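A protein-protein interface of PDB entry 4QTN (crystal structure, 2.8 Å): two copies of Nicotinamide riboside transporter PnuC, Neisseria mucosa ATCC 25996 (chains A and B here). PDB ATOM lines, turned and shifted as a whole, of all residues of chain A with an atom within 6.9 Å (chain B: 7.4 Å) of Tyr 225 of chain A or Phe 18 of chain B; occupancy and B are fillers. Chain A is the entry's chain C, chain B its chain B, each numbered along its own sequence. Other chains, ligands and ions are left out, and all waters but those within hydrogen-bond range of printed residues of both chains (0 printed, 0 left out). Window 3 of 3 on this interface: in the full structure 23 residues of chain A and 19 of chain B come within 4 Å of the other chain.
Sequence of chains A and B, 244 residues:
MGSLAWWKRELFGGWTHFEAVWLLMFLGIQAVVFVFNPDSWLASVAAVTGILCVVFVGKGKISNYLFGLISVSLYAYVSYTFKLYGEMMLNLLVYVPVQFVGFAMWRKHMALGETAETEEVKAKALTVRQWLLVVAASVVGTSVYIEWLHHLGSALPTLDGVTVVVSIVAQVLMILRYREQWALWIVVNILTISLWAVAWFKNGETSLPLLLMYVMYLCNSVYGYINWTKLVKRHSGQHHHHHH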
ATOM      1  N   GLY A  58      19.766 -11.111 -29.958  1.00  0.00           N
ATOM      2  CA  GLY A  58      19.607  -9.954 -29.090  1.00  0.00           C
ATOM      3  C   GLY A  58      19.343 -10.379 -27.672  1.00  0.00           C
ATOM      4  O   GLY A  58      19.857  -9.779 -26.732  1.00  0.00           O
ATOM      5  N   VAL A 128      38.703  -0.054 -25.763  1.00  0.00           N
ATOM      6  CA  VAL A 128      38.864   0.855 -26.878  1.00  0.00           C
ATOM      7  C   VAL A 128      40.087   0.424 -27.686  1.00  0.00           C
ATOM      8  O   VAL A 128      40.071   0.416 -28.938  1.00  0.00           O
ATOM      9  CB  VAL A 128      39.041   2.312 -26.386  1.00  0.00           C
ATOM     10  CG1 VAL A 128      38.987   3.283 -27.550  1.00  0.00           C
ATOM     11  CG2 VAL A 128      37.981   2.669 -25.344  1.00  0.00           C
ATOM     12  N   ARG A 179      29.840  -7.605 -27.088  1.00  0.00           N
ATOM     13  CA  ARG A 179      28.737  -6.667 -27.233  1.00  0.00           C
ATOM     14  C   ARG A 179      28.950  -5.636 -28.353  1.00  0.00           C
ATOM     15  O   ARG A 179      28.013  -5.029 -28.802  1.00  0.00           O
ATOM     16  CB  ARG A 179      28.466  -5.953 -25.926  1.00  0.00           C
ATOM     17  CG  ARG A 179      28.073  -4.511 -26.123  1.00  0.00           C
ATOM     18  CD  ARG A 179      27.535  -3.917 -24.857  1.00  0.00           C
ATOM     19  NE  ARG A 179      28.596  -3.592 -23.920  1.00  0.00           N
ATOM     20  CZ  ARG A 179      29.440  -2.580 -24.071  1.00  0.00           C
ATOM     21  NH1 ARG A 179      29.365  -1.790 -25.147  1.00  0.00           N
ATOM     22  NH2 ARG A 179      30.371  -2.359 -23.153  1.00  0.00           N
ATOM     23  N   GLU A 180      30.183  -5.426 -28.787  1.00  0.00           N
ATOM     24  CA  GLU A 180      30.438  -4.377 -29.792  1.00  0.00           C
ATOM     25  C   GLU A 180      29.940  -4.765 -31.189  1.00  0.00           C
ATOM     26  O   GLU A 180      29.926  -3.939 -32.105  1.00  0.00           O
ATOM     27  CB  GLU A 180      31.917  -3.972 -29.812  1.00  0.00           C
ATOM     28  CG  GLU A 180      32.330  -3.086 -28.627  1.00  0.00           C
ATOM     29  CD  GLU A 180      32.199  -3.793 -27.277  1.00  0.00           C
ATOM     30  OE1 GLU A 180      32.314  -5.037 -27.250  1.00  0.00           O
ATOM     31  OE2 GLU A 180      31.984  -3.103 -26.246  1.00  0.00           O
ATOM     32  N   GLN A 181      29.515  -6.021 -31.334  1.00  0.00           N
ATOM     33  CA  GLN A 181      28.965  -6.513 -32.582  1.00  0.00           C
ATOM     34  C   GLN A 181      27.781  -5.637 -33.024  1.00  0.00           C
ATOM     35  O   GLN A 181      27.687  -5.256 -34.184  1.00  0.00           O
ATOM     36  CB  GLN A 181      28.520  -7.963 -32.420  1.00  0.00           C
ATOM     37  CG  GLN A 181      27.496  -8.161 -31.299  1.00  0.00           C
ATOM     38  CD  GLN A 181      26.708  -9.444 -31.438  1.00  0.00           C
ATOM     39  OE1 GLN A 181      26.094  -9.698 -32.474  1.00  0.00           O
ATOM     40  NE2 GLN A 181      26.723 -10.265 -30.393  1.00  0.00           N
ATOM     41  N   TRP A 182      26.910  -5.290 -32.073  1.00  0.00           N
ATOM     42  CA  TRP A 182      25.741  -4.446 -32.350  1.00  0.00           C
ATOM     43  C   TRP A 182      26.021  -3.067 -32.958  1.00  0.00           C
ATOM     44  O   TRP A 182      25.228  -2.572 -33.750  1.00  0.00           O
ATOM     45  CB  TRP A 182      24.845  -4.328 -31.120  1.00  0.00           C
ATOM     46  CG  TRP A 182      24.362  -5.654 -30.661  1.00  0.00           C
ATOM     47  CD1 TRP A 182      24.824  -6.355 -29.603  1.00  0.00           C
ATOM     48  CD2 TRP A 182      23.363  -6.480 -31.286  1.00  0.00           C
ATOM     49  NE1 TRP A 182      24.162  -7.550 -29.496  1.00  0.00           N
ATOM     50  CE2 TRP A 182      23.258  -7.652 -30.520  1.00  0.00           C
ATOM     51  CE3 TRP A 182      22.534  -6.330 -32.401  1.00  0.00           C
ATOM     52  CZ2 TRP A 182      22.368  -8.682 -30.838  1.00  0.00           C
ATOM     53  CZ3 TRP A 182      21.653  -7.353 -32.715  1.00  0.00           C
ATOM     54  CH2 TRP A 182      21.589  -8.518 -31.943  1.00  0.00           C
ATOM     55  N   ALA A 183      27.131  -2.439 -32.598  1.00  0.00           N
ATOM     56  CA  ALA A 183      27.487  -1.211 -33.280  1.00  0.00           C
ATOM     57  C   ALA A 183      27.652  -1.505 -34.767  1.00  0.00           C
ATOM     58  O   ALA A 183      27.107  -0.788 -35.601  1.00  0.00           O
ATOM     59  CB  ALA A 183      28.732  -0.603 -32.695  1.00  0.00           C
ATOM     60  N   LEU A 184      28.340  -2.614 -35.084  1.00  0.00           N
ATOM     61  CA  LEU A 184      28.527  -3.056 -36.476  1.00  0.00           C
ATOM     62  C   LEU A 184      27.221  -3.449 -37.127  1.00  0.00           C
ATOM     63  O   LEU A 184      26.886  -2.928 -38.175  1.00  0.00           O
ATOM     64  CB  LEU A 184      29.515  -4.215 -36.571  1.00  0.00           C
ATOM     65  CG  LEU A 184      31.001  -3.935 -36.776  1.00  0.00           C
ATOM     66  CD1 LEU A 184      31.244  -2.871 -37.832  1.00  0.00           C
ATOM     67  CD2 LEU A 184      31.631  -3.532 -35.471  1.00  0.00           C
ATOM     68  N   ILE A 186      24.327  -2.397 -36.640  1.00  0.00           N
ATOM     69  CA  ILE A 186      23.554  -1.202 -37.022  1.00  0.00           C
ATOM     70  C   ILE A 186      24.001  -0.640 -38.382  1.00  0.00           C
ATOM     71  O   ILE A 186      23.179  -0.232 -39.194  1.00  0.00           O
ATOM     72  CB  ILE A 186      23.497  -0.115 -35.911  1.00  0.00           C
ATOM     73  CG1 ILE A 186      22.474  -0.514 -34.863  1.00  0.00           C
ATOM     74  CG2 ILE A 186      23.019   1.212 -36.483  1.00  0.00           C
ATOM     75  CD1 ILE A 186      22.900  -0.251 -33.453  1.00  0.00           C
ATOM     76  N   ASN A 220      15.629  -4.033 -34.154  1.00  0.00           N
ATOM     77  CA  ASN A 220      16.132  -5.048 -33.239  1.00  0.00           C
ATOM     78  C   ASN A 220      17.617  -4.885 -32.925  1.00  0.00           C
ATOM     79  O   ASN A 220      18.048  -5.138 -31.804  1.00  0.00           O
ATOM     80  CB  ASN A 220      15.838  -6.437 -33.803  1.00  0.00           C
ATOM     81  CG  ASN A 220      16.655  -7.534 -33.136  1.00  0.00           C
ATOM     82  OD1 ASN A 220      16.308  -8.009 -32.034  1.00  0.00           O
ATOM     83  ND2 ASN A 220      17.750  -7.973 -33.817  1.00  0.00           N
ATOM     84  N   SER A 221      18.400  -4.463 -33.913  1.00  0.00           N
ATOM     85  CA  SER A 221      19.826  -4.277 -33.691  1.00  0.00           C
ATOM     86  C   SER A 221      20.111  -3.117 -32.724  1.00  0.00           C
ATOM     87  O   SER A 221      21.154  -3.103 -32.075  1.00  0.00           O
ATOM     88  CB  SER A 221      20.600  -4.131 -35.016  1.00  0.00           C
ATOM     89  OG  SER A 221      20.472  -2.827 -35.555  1.00  0.00           O
ATOM     90  N   VAL A 222      19.165  -2.173 -32.587  1.00  0.00           N
ATOM     91  CA  VAL A 222      19.275  -1.198 -31.501  1.00  0.00           C
ATOM     92  C   VAL A 222      18.894  -1.841 -30.189  1.00  0.00           C
ATOM     93  O   VAL A 222      19.582  -1.657 -29.189  1.00  0.00           O
ATOM     94  CB  VAL A 222      18.459   0.088 -31.721  1.00  0.00           C
ATOM     95  CG1 VAL A 222      18.181   0.759 -30.385  1.00  0.00           C
ATOM     96  CG2 VAL A 222      19.220   1.048 -32.605  1.00  0.00           C
ATOM     97  N   TYR A 223      17.832  -2.643 -30.192  1.00  0.00           N
ATOM     98  CA  TYR A 223      17.514  -3.451 -28.999  1.00  0.00           C
ATOM     99  C   TYR A 223      18.697  -4.313 -28.543  1.00  0.00           C
ATOM    100  O   TYR A 223      19.035  -4.330 -27.361  1.00  0.00           O
ATOM    101  CB  TYR A 223      16.319  -4.350 -29.229  1.00  0.00           C
ATOM    102  CG  TYR A 223      15.838  -4.967 -27.958  1.00  0.00           C
ATOM    103  CD1 TYR A 223      15.332  -4.159 -26.932  1.00  0.00           C
ATOM    104  CD2 TYR A 223      15.925  -6.354 -27.739  1.00  0.00           C
ATOM    105  CE1 TYR A 223      14.896  -4.692 -25.742  1.00  0.00           C
ATOM    106  CE2 TYR A 223      15.480  -6.912 -26.535  1.00  0.00           C
ATOM    107  CZ  TYR A 223      14.961  -6.062 -25.542  1.00  0.00           C
ATOM    108  OH  TYR A 223      14.516  -6.551 -24.351  1.00  0.00           O
ATOM    109  N   GLY A 224      19.297  -5.045 -29.491  1.00  0.00           N
ATOM    110  CA  GLY A 224      20.478  -5.883 -29.229  1.00  0.00           C
ATOM    111  C   GLY A 224      21.567  -5.150 -28.467  1.00  0.00           C
ATOM    112  O   GLY A 224      21.981  -5.571 -27.383  1.00  0.00           O
ATOM    113  N   TYR A 225      21.999  -4.028 -29.006  1.00  0.00           N
ATOM    114  CA  TYR A 225      22.969  -3.207 -28.322  1.00  0.00           C
ATOM    115  C   TYR A 225      22.540  -2.906 -26.880  1.00  0.00           C
ATOM    116  O   TYR A 225      23.286  -3.199 -25.931  1.00  0.00           O
ATOM    117  CB  TYR A 225      23.217  -1.936 -29.090  1.00  0.00           C
ATOM    118  CG  TYR A 225      24.570  -1.344 -28.872  1.00  0.00           C
ATOM    119  CD1 TYR A 225      25.104  -1.259 -27.616  1.00  0.00           C
ATOM    120  CD2 TYR A 225      25.293  -0.806 -29.926  1.00  0.00           C
ATOM    121  CE1 TYR A 225      26.335  -0.669 -27.395  1.00  0.00           C
ATOM    122  CE2 TYR A 225      26.524  -0.191 -29.716  1.00  0.00           C
ATOM    123  CZ  TYR A 225      27.039  -0.131 -28.442  1.00  0.00           C
ATOM    124  OH  TYR A 225      28.271   0.453 -28.200  1.00  0.00           O
ATOM    125  N   ILE A 226      21.325  -2.387 -26.705  1.00  0.00           N
ATOM    126  CA  ILE A 226      20.786  -2.152 -25.339  1.00  0.00           C
ATOM    127  C   ILE A 226      20.810  -3.405 -24.427  1.00  0.00           C
ATOM    128  O   ILE A 226      21.384  -3.362 -23.334  1.00  0.00           O
ATOM    129  CB  ILE A 226      19.379  -1.558 -25.359  1.00  0.00           C
ATOM    130  CG1 ILE A 226      19.438  -0.083 -25.671  1.00  0.00           C
ATOM    131  CG2 ILE A 226      18.734  -1.711 -24.011  1.00  0.00           C
ATOM    132  CD1 ILE A 226      18.363   0.359 -26.633  1.00  0.00           C
ATOM    133  N   ASN A 227      20.220  -4.511 -24.896  1.00  0.00           N
ATOM    134  CA  ASN A 227      20.081  -5.728 -24.088  1.00  0.00           C
ATOM    135  C   ASN A 227      21.375  -6.410 -23.803  1.00  0.00           C
ATOM    136  O   ASN A 227      21.597  -6.883 -22.682  1.00  0.00           O
ATOM    137  CB  ASN A 227      19.169  -6.729 -24.762  1.00  0.00           C
ATOM    138  CG  ASN A 227      18.689  -7.809 -23.805  1.00  0.00           C
ATOM    139  OD1 ASN A 227      17.938  -7.527 -22.851  1.00  0.00           O
ATOM    140  ND2 ASN A 227      19.110  -9.055 -24.049  1.00  0.00           N
ATOM    141  N   TRP A 228      22.205  -6.546 -24.836  1.00  0.00           N
ATOM    142  CA  TRP A 228      23.571  -7.042 -24.662  1.00  0.00           C
ATOM    143  C   TRP A 228      24.412  -6.211 -23.686  1.00  0.00           C
ATOM    144  O   TRP A 228      25.252  -6.761 -22.980  1.00  0.00           O
ATOM    145  CB  TRP A 228      24.278  -7.212 -26.004  1.00  0.00           C
ATOM    146  CG  TRP A 228      24.083  -8.538 -26.532  1.00  0.00           C
ATOM    147  CD1 TRP A 228      22.899  -9.119 -26.833  1.00  0.00           C
ATOM    148  CD2 TRP A 228      25.091  -9.517 -26.785  1.00  0.00           C
ATOM    149  NE1 TRP A 228      23.093 -10.409 -27.272  1.00  0.00           N
ATOM    150  CE2 TRP A 228      24.434 -10.679 -27.254  1.00  0.00           C
ATOM    151  CE3 TRP A 228      26.484  -9.526 -26.683  1.00  0.00           C
ATOM    152  CZ2 TRP A 228      25.126 -11.838 -27.617  1.00  0.00           C
ATOM    153  CZ3 TRP A 228      27.174 -10.690 -27.036  1.00  0.00           C
ATOM    154  CH2 TRP A 228      26.492 -11.824 -27.495  1.00  0.00           C
ATOM    155  N   THR A 229      24.168  -4.907 -23.602  1.00  0.00           N
ATOM    156  CA  THR A 229      24.758  -4.153 -22.509  1.00  0.00           C
ATOM    157  C   THR A 229      24.305  -4.678 -21.142  1.00  0.00           C
ATOM    158  O   THR A 229      25.142  -5.001 -20.291  1.00  0.00           O
ATOM    159  CB  THR A 229      24.525  -2.650 -22.627  1.00  0.00           C
ATOM    160  OG1 THR A 229      25.247  -2.170 -23.749  1.00  0.00           O
ATOM    161  CG2 THR A 229      25.050  -1.945 -21.405  1.00  0.00           C
ATOM    162  N   LYS A 230      22.991  -4.780 -20.940  1.00  0.00           N
ATOM    163  CA  LYS A 230      22.451  -5.336 -19.690  1.00  0.00           C
ATOM    164  C   LYS A 230      23.102  -6.700 -19.388  1.00  0.00           C
ATOM    165  O   LYS A 230      23.362  -7.038 -18.229  1.00  0.00           O
ATOM    166  CB  LYS A 230      20.909  -5.443 -19.743  1.00  0.00           C
ATOM    167  CG  LYS A 230      20.188  -4.089 -19.624  1.00  0.00           C
ATOM    168  CD  LYS A 230      18.893  -4.024 -20.468  1.00  0.00           C
ATOM    169  CE  LYS A 230      17.634  -4.390 -19.672  1.00  0.00           C
ATOM    170  NZ  LYS A 230      16.814  -3.204 -19.275  1.00  0.00           N
ATOM    171  N   TRP B  15      37.051  10.750 -23.338  1.00  0.00           N
ATOM    172  CA  TRP B  15      36.056  10.028 -24.121  1.00  0.00           C
ATOM    173  C   TRP B  15      35.528   8.895 -23.292  1.00  0.00           C
ATOM    174  O   TRP B  15      36.286   8.197 -22.625  1.00  0.00           O
ATOM    175  CB  TRP B  15      36.677   9.428 -25.389  1.00  0.00           C
ATOM    176  CG  TRP B  15      37.184  10.434 -26.389  1.00  0.00           C
ATOM    177  CD1 TRP B  15      38.485  10.712 -26.670  1.00  0.00           C
ATOM    178  CD2 TRP B  15      36.394  11.268 -27.272  1.00  0.00           C
ATOM    179  NE1 TRP B  15      38.560  11.687 -27.634  1.00  0.00           N
ATOM    180  CE2 TRP B  15      37.293  12.044 -28.021  1.00  0.00           C
ATOM    181  CE3 TRP B  15      35.015  11.450 -27.474  1.00  0.00           C
ATOM    182  CZ2 TRP B  15      36.866  12.991 -28.965  1.00  0.00           C
ATOM    183  CZ3 TRP B  15      34.592  12.390 -28.418  1.00  0.00           C
ATOM    184  CH2 TRP B  15      35.511  13.148 -29.144  1.00  0.00           C
ATOM    185  N   THR B  16      34.222   8.688 -23.341  1.00  0.00           N
ATOM    186  CA  THR B  16      33.622   7.487 -22.751  1.00  0.00           C
ATOM    187  C   THR B  16      33.939   6.299 -23.647  1.00  0.00           C
ATOM    188  O   THR B  16      34.279   6.487 -24.826  1.00  0.00           O
ATOM    189  CB  THR B  16      32.104   7.635 -22.625  1.00  0.00           C
ATOM    190  OG1 THR B  16      31.518   7.785 -23.941  1.00  0.00           O
ATOM    191  CG2 THR B  16      31.760   8.855 -21.743  1.00  0.00           C
ATOM    192  N   HIS B  17      33.837   5.082 -23.102  1.00  0.00           N
ATOM    193  CA  HIS B  17      34.052   3.885 -23.913  1.00  0.00           C
ATOM    194  C   HIS B  17      33.128   3.894 -25.102  1.00  0.00           C
ATOM    195  O   HIS B  17      33.544   3.566 -26.212  1.00  0.00           O
ATOM    196  CB  HIS B  17      33.830   2.632 -23.108  1.00  0.00           C
ATOM    197  CG  HIS B  17      33.983   1.373 -23.904  1.00  0.00           C
ATOM    198  ND1 HIS B  17      32.965   0.847 -24.676  1.00  0.00           N
ATOM    199  CD2 HIS B  17      35.031   0.526 -24.040  1.00  0.00           C
ATOM    200  CE1 HIS B  17      33.379  -0.266 -25.253  1.00  0.00           C
ATOM    201  NE2 HIS B  17      34.629  -0.483 -24.884  1.00  0.00           N
ATOM    202  N   PHE B  18      31.865   4.285 -24.859  1.00  0.00           N
ATOM    203  CA  PHE B  18      30.837   4.423 -25.916  1.00  0.00           C
ATOM    204  C   PHE B  18      31.219   5.376 -27.072  1.00  0.00           C
ATOM    205  O   PHE B  18      31.351   4.924 -28.241  1.00  0.00           O
ATOM    206  CB  PHE B  18      29.477   4.832 -25.319  1.00  0.00           C
ATOM    207  CG  PHE B  18      28.333   4.702 -26.287  1.00  0.00           C
ATOM    208  CD1 PHE B  18      27.796   3.443 -26.593  1.00  0.00           C
ATOM    209  CD2 PHE B  18      27.822   5.826 -26.938  1.00  0.00           C
ATOM    210  CE1 PHE B  18      26.758   3.319 -27.513  1.00  0.00           C
ATOM    211  CE2 PHE B  18      26.787   5.704 -27.865  1.00  0.00           C
ATOM    212  CZ  PHE B  18      26.251   4.452 -28.144  1.00  0.00           C
ATOM    213  N   GLU B  19      31.366   6.684 -26.753  1.00  0.00           N
ATOM    214  CA  GLU B  19      31.798   7.698 -27.733  1.00  0.00           C
ATOM    215  C   GLU B  19      32.979   7.176 -28.523  1.00  0.00           C
ATOM    216  O   GLU B  19      33.016   7.288 -29.737  1.00  0.00           O
ATOM    217  CB  GLU B  19      32.218   8.985 -27.040  1.00  0.00           C
ATOM    218  CG  GLU B  19      31.120   9.737 -26.337  1.00  0.00           C
ATOM    219  CD  GLU B  19      31.643  10.635 -25.210  1.00  0.00           C
ATOM    220  OE1 GLU B  19      30.817  11.161 -24.421  1.00  0.00           O
ATOM    221  OE2 GLU B  19      32.867  10.815 -25.106  1.00  0.00           O
ATOM    222  N   ALA B  20      33.958   6.620 -27.814  1.00  0.00           N
ATOM    223  CA  ALA B  20      35.138   6.069 -28.437  1.00  0.00           C
ATOM    224  C   ALA B  20      34.787   4.972 -29.408  1.00  0.00           C
ATOM    225  O   ALA B  20      35.204   5.009 -30.576  1.00  0.00           O
ATOM    226  CB  ALA B  20      36.083   5.546 -27.389  1.00  0.00           C
ATOM    227  N   VAL B  21      34.017   3.988 -28.938  1.00  0.00           N
ATOM    228  CA  VAL B  21      33.708   2.842 -29.757  1.00  0.00           C
ATOM    229  C   VAL B  21      33.018   3.253 -31.023  1.00  0.00           C
ATOM    230  O   VAL B  21      33.251   2.659 -32.069  1.00  0.00           O
ATOM    231  CB  VAL B  21      32.863   1.799 -29.030  1.00  0.00           C
ATOM    232  CG1 VAL B  21      31.986   1.040 -30.024  1.00  0.00           C
ATOM    233  CG2 VAL B  21      33.769   0.824 -28.288  1.00  0.00           C
ATOM    234  N   TRP B  22      32.202   4.297 -30.951  1.00  0.00           N
ATOM    235  CA  TRP B  22      31.481   4.753 -32.144  1.00  0.00           C
ATOM    236  C   TRP B  22      32.314   5.627 -33.098  1.00  0.00           C
ATOM    237  O   TRP B  22      32.417   5.348 -34.296  1.00  0.00           O
ATOM    238  CB  TRP B  22      30.172   5.436 -31.763  1.00  0.00           C
ATOM    239  CG  TRP B  22      29.105   4.462 -31.511  1.00  0.00           C
ATOM    240  CD1 TRP B  22      28.811   3.852 -30.318  1.00  0.00           C
ATOM    241  CD2 TRP B  22      28.216   3.918 -32.472  1.00  0.00           C
ATOM    242  NE1 TRP B  22      27.770   2.975 -30.480  1.00  0.00           N
ATOM    243  CE2 TRP B  22      27.384   2.991 -31.795  1.00  0.00           C
ATOM    244  CE3 TRP B  22      28.036   4.115 -33.845  1.00  0.00           C
ATOM    245  CZ2 TRP B  22      26.383   2.270 -32.445  1.00  0.00           C
ATOM    246  CZ3 TRP B  22      27.037   3.402 -34.492  1.00  0.00           C
ATOM    247  CH2 TRP B  22      26.218   2.490 -33.788  1.00  0.00           C
ATOM    248  N   LEU B  23      32.890   6.688 -32.573  1.00  0.00           N
ATOM    249  CA  LEU B  23      33.676   7.557 -33.391  1.00  0.00           C
ATOM    250  C   LEU B  23      34.766   6.777 -34.161  1.00  0.00           C
ATOM    251  O   LEU B  23      35.075   7.107 -35.306  1.00  0.00           O
ATOM    252  CB  LEU B  23      34.269   8.672 -32.549  1.00  0.00           C
ATOM    253  CG  LEU B  23      35.503   9.389 -33.043  1.00  0.00           C
ATOM    254  CD1 LEU B  23      35.178  10.274 -34.229  1.00  0.00           C
ATOM    255  CD2 LEU B  23      36.029  10.203 -31.883  1.00  0.00           C
ATOM    256  N   LEU B  24      35.308   5.721 -33.555  1.00  0.00           N
ATOM    257  CA  LEU B  24      36.267   4.889 -34.275  1.00  0.00           C
ATOM    258  C   LEU B  24      35.592   4.080 -35.372  1.00  0.00           C
ATOM    259  O   LEU B  24      36.042   4.078 -36.502  1.00  0.00           O
ATOM    260  CB  LEU B  24      37.052   3.972 -33.334  1.00  0.00           C
ATOM    261  CG  LEU B  24      38.086   4.560 -32.348  1.00  0.00           C
ATOM    262  CD1 LEU B  24      38.860   3.424 -31.673  1.00  0.00           C
ATOM    263  CD2 LEU B  24      39.046   5.563 -32.996  1.00  0.00           C
ATOM    264  N   TYR B 223      23.058  11.674 -30.192  1.00  0.00           N
ATOM    265  CA  TYR B 223      24.059  11.783 -29.123  1.00  0.00           C
ATOM    266  C   TYR B 223      24.311  13.225 -28.757  1.00  0.00           C
ATOM    267  O   TYR B 223      24.461  13.556 -27.594  1.00  0.00           O
ATOM    268  CB  TYR B 223      25.382  11.147 -29.497  1.00  0.00           C
ATOM    269  CG  TYR B 223      26.266  10.983 -28.285  1.00  0.00           C
ATOM    270  CD1 TYR B 223      26.032   9.953 -27.383  1.00  0.00           C
ATOM    271  CD2 TYR B 223      27.290  11.918 -27.985  1.00  0.00           C
ATOM    272  CE1 TYR B 223      26.799   9.806 -26.245  1.00  0.00           C
ATOM    273  CE2 TYR B 223      28.062  11.786 -26.837  1.00  0.00           C
ATOM    274  CZ  TYR B 223      27.806  10.718 -25.962  1.00  0.00           C
ATOM    275  OH  TYR B 223      28.558  10.521 -24.807  1.00  0.00           O
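The indole nitrogen (NE1) of Trp 22 of chain B is in hydrogen-bond range of the side-chain hydroxyl (OH) of Tyr 225 of chain A, 3.4 Å away.
The side-chain carboxylate (OE2) of Glu 180 of chain A is in salt-bridge range of the guanidinium group (NH1) of Arg 179 of chain A, 3.1 Å away. The side-chain hydroxyl (OG1) of Thr 229 of chain A lies within hydrogen-bond range of the backbone carbonyl oxygen (O) of Tyr 225 of chain A.
Val 128 of chain A touches His 17 of chain B. CB of Ala 20 of chain B touches CG1 of Val 128 of chain A (3.7 Å). His 17 of chain B touches Glu 180 of chain A (CE1 to OE2, 3.3 Å). Ala 183 of chain A touches Trp 22 of chain B. OH of Tyr 225 of chain A touches CE1 of Phe 18 of chain B, at 3.3 Å.
Of chain B, only Phe 18 (3.3 Å) and Trp 22 (3.4 Å) come within 4 Å of Tyr 225 of chain A. Phe 18 of chain B touches one residue of chain A. No residue of chain B comes within 4 Å of Gly 224 of chain A. Printed residues of chain A within 4 Å of Ala 20 of chain B: Val 128. Of the printed residues of chain B, Glu 180 of chain A touches His 17. Printed residues of chain A within 4 Å of His 17 of chain B: Val 128 (3.9 Å) and Glu 180 (3.3 Å). Of the printed residues of chain B, Val 128 of chain A touches His 17 (3.9 Å) and Ala 20 (3.7 Å). Printed residues of chain A within 4 Å of Trp 22 of chain B: Ala 183 and Tyr 225. The nearest residue of chain B that does not touch Tyr 225 of chain A is Val 21 of chain B (4.2 Å). The nearest residue of chain A that does not touch Phe 18 of chain B is Arg 179 of chain A (5.7 Å). The nearest printed residue of chain A that does not touch Ala 20 of chain B is Tyr 225 of chain A (8.0 Å).
Of the 20 printed residues of chain A, 4 touch a printed residue of chain B. Hydrophobic or aromatic side chains of chain A that line the printed part of chain B: Val 128, Ala 183 and Tyr 225. Along chain A the printed residues that touch a printed residue of chain B span positions 128 to 225. Hydrophobic or aromatic side chains of chain B within 4 Å of the printed part of chain A: His 17, Phe 18, Ala 20 and Trp 22. Among the printed residues, 6 pairs touch across the chains. Among the printed residues, no Asp or Glu carboxylate lies within 4 Å of a Lys or Arg side-chain nitrogen of the other chain.
Position printed for both chains: 223. Of the 6 pairs that touch across the chains among the printed residues, none has its exchanged pair printed and touching as well.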
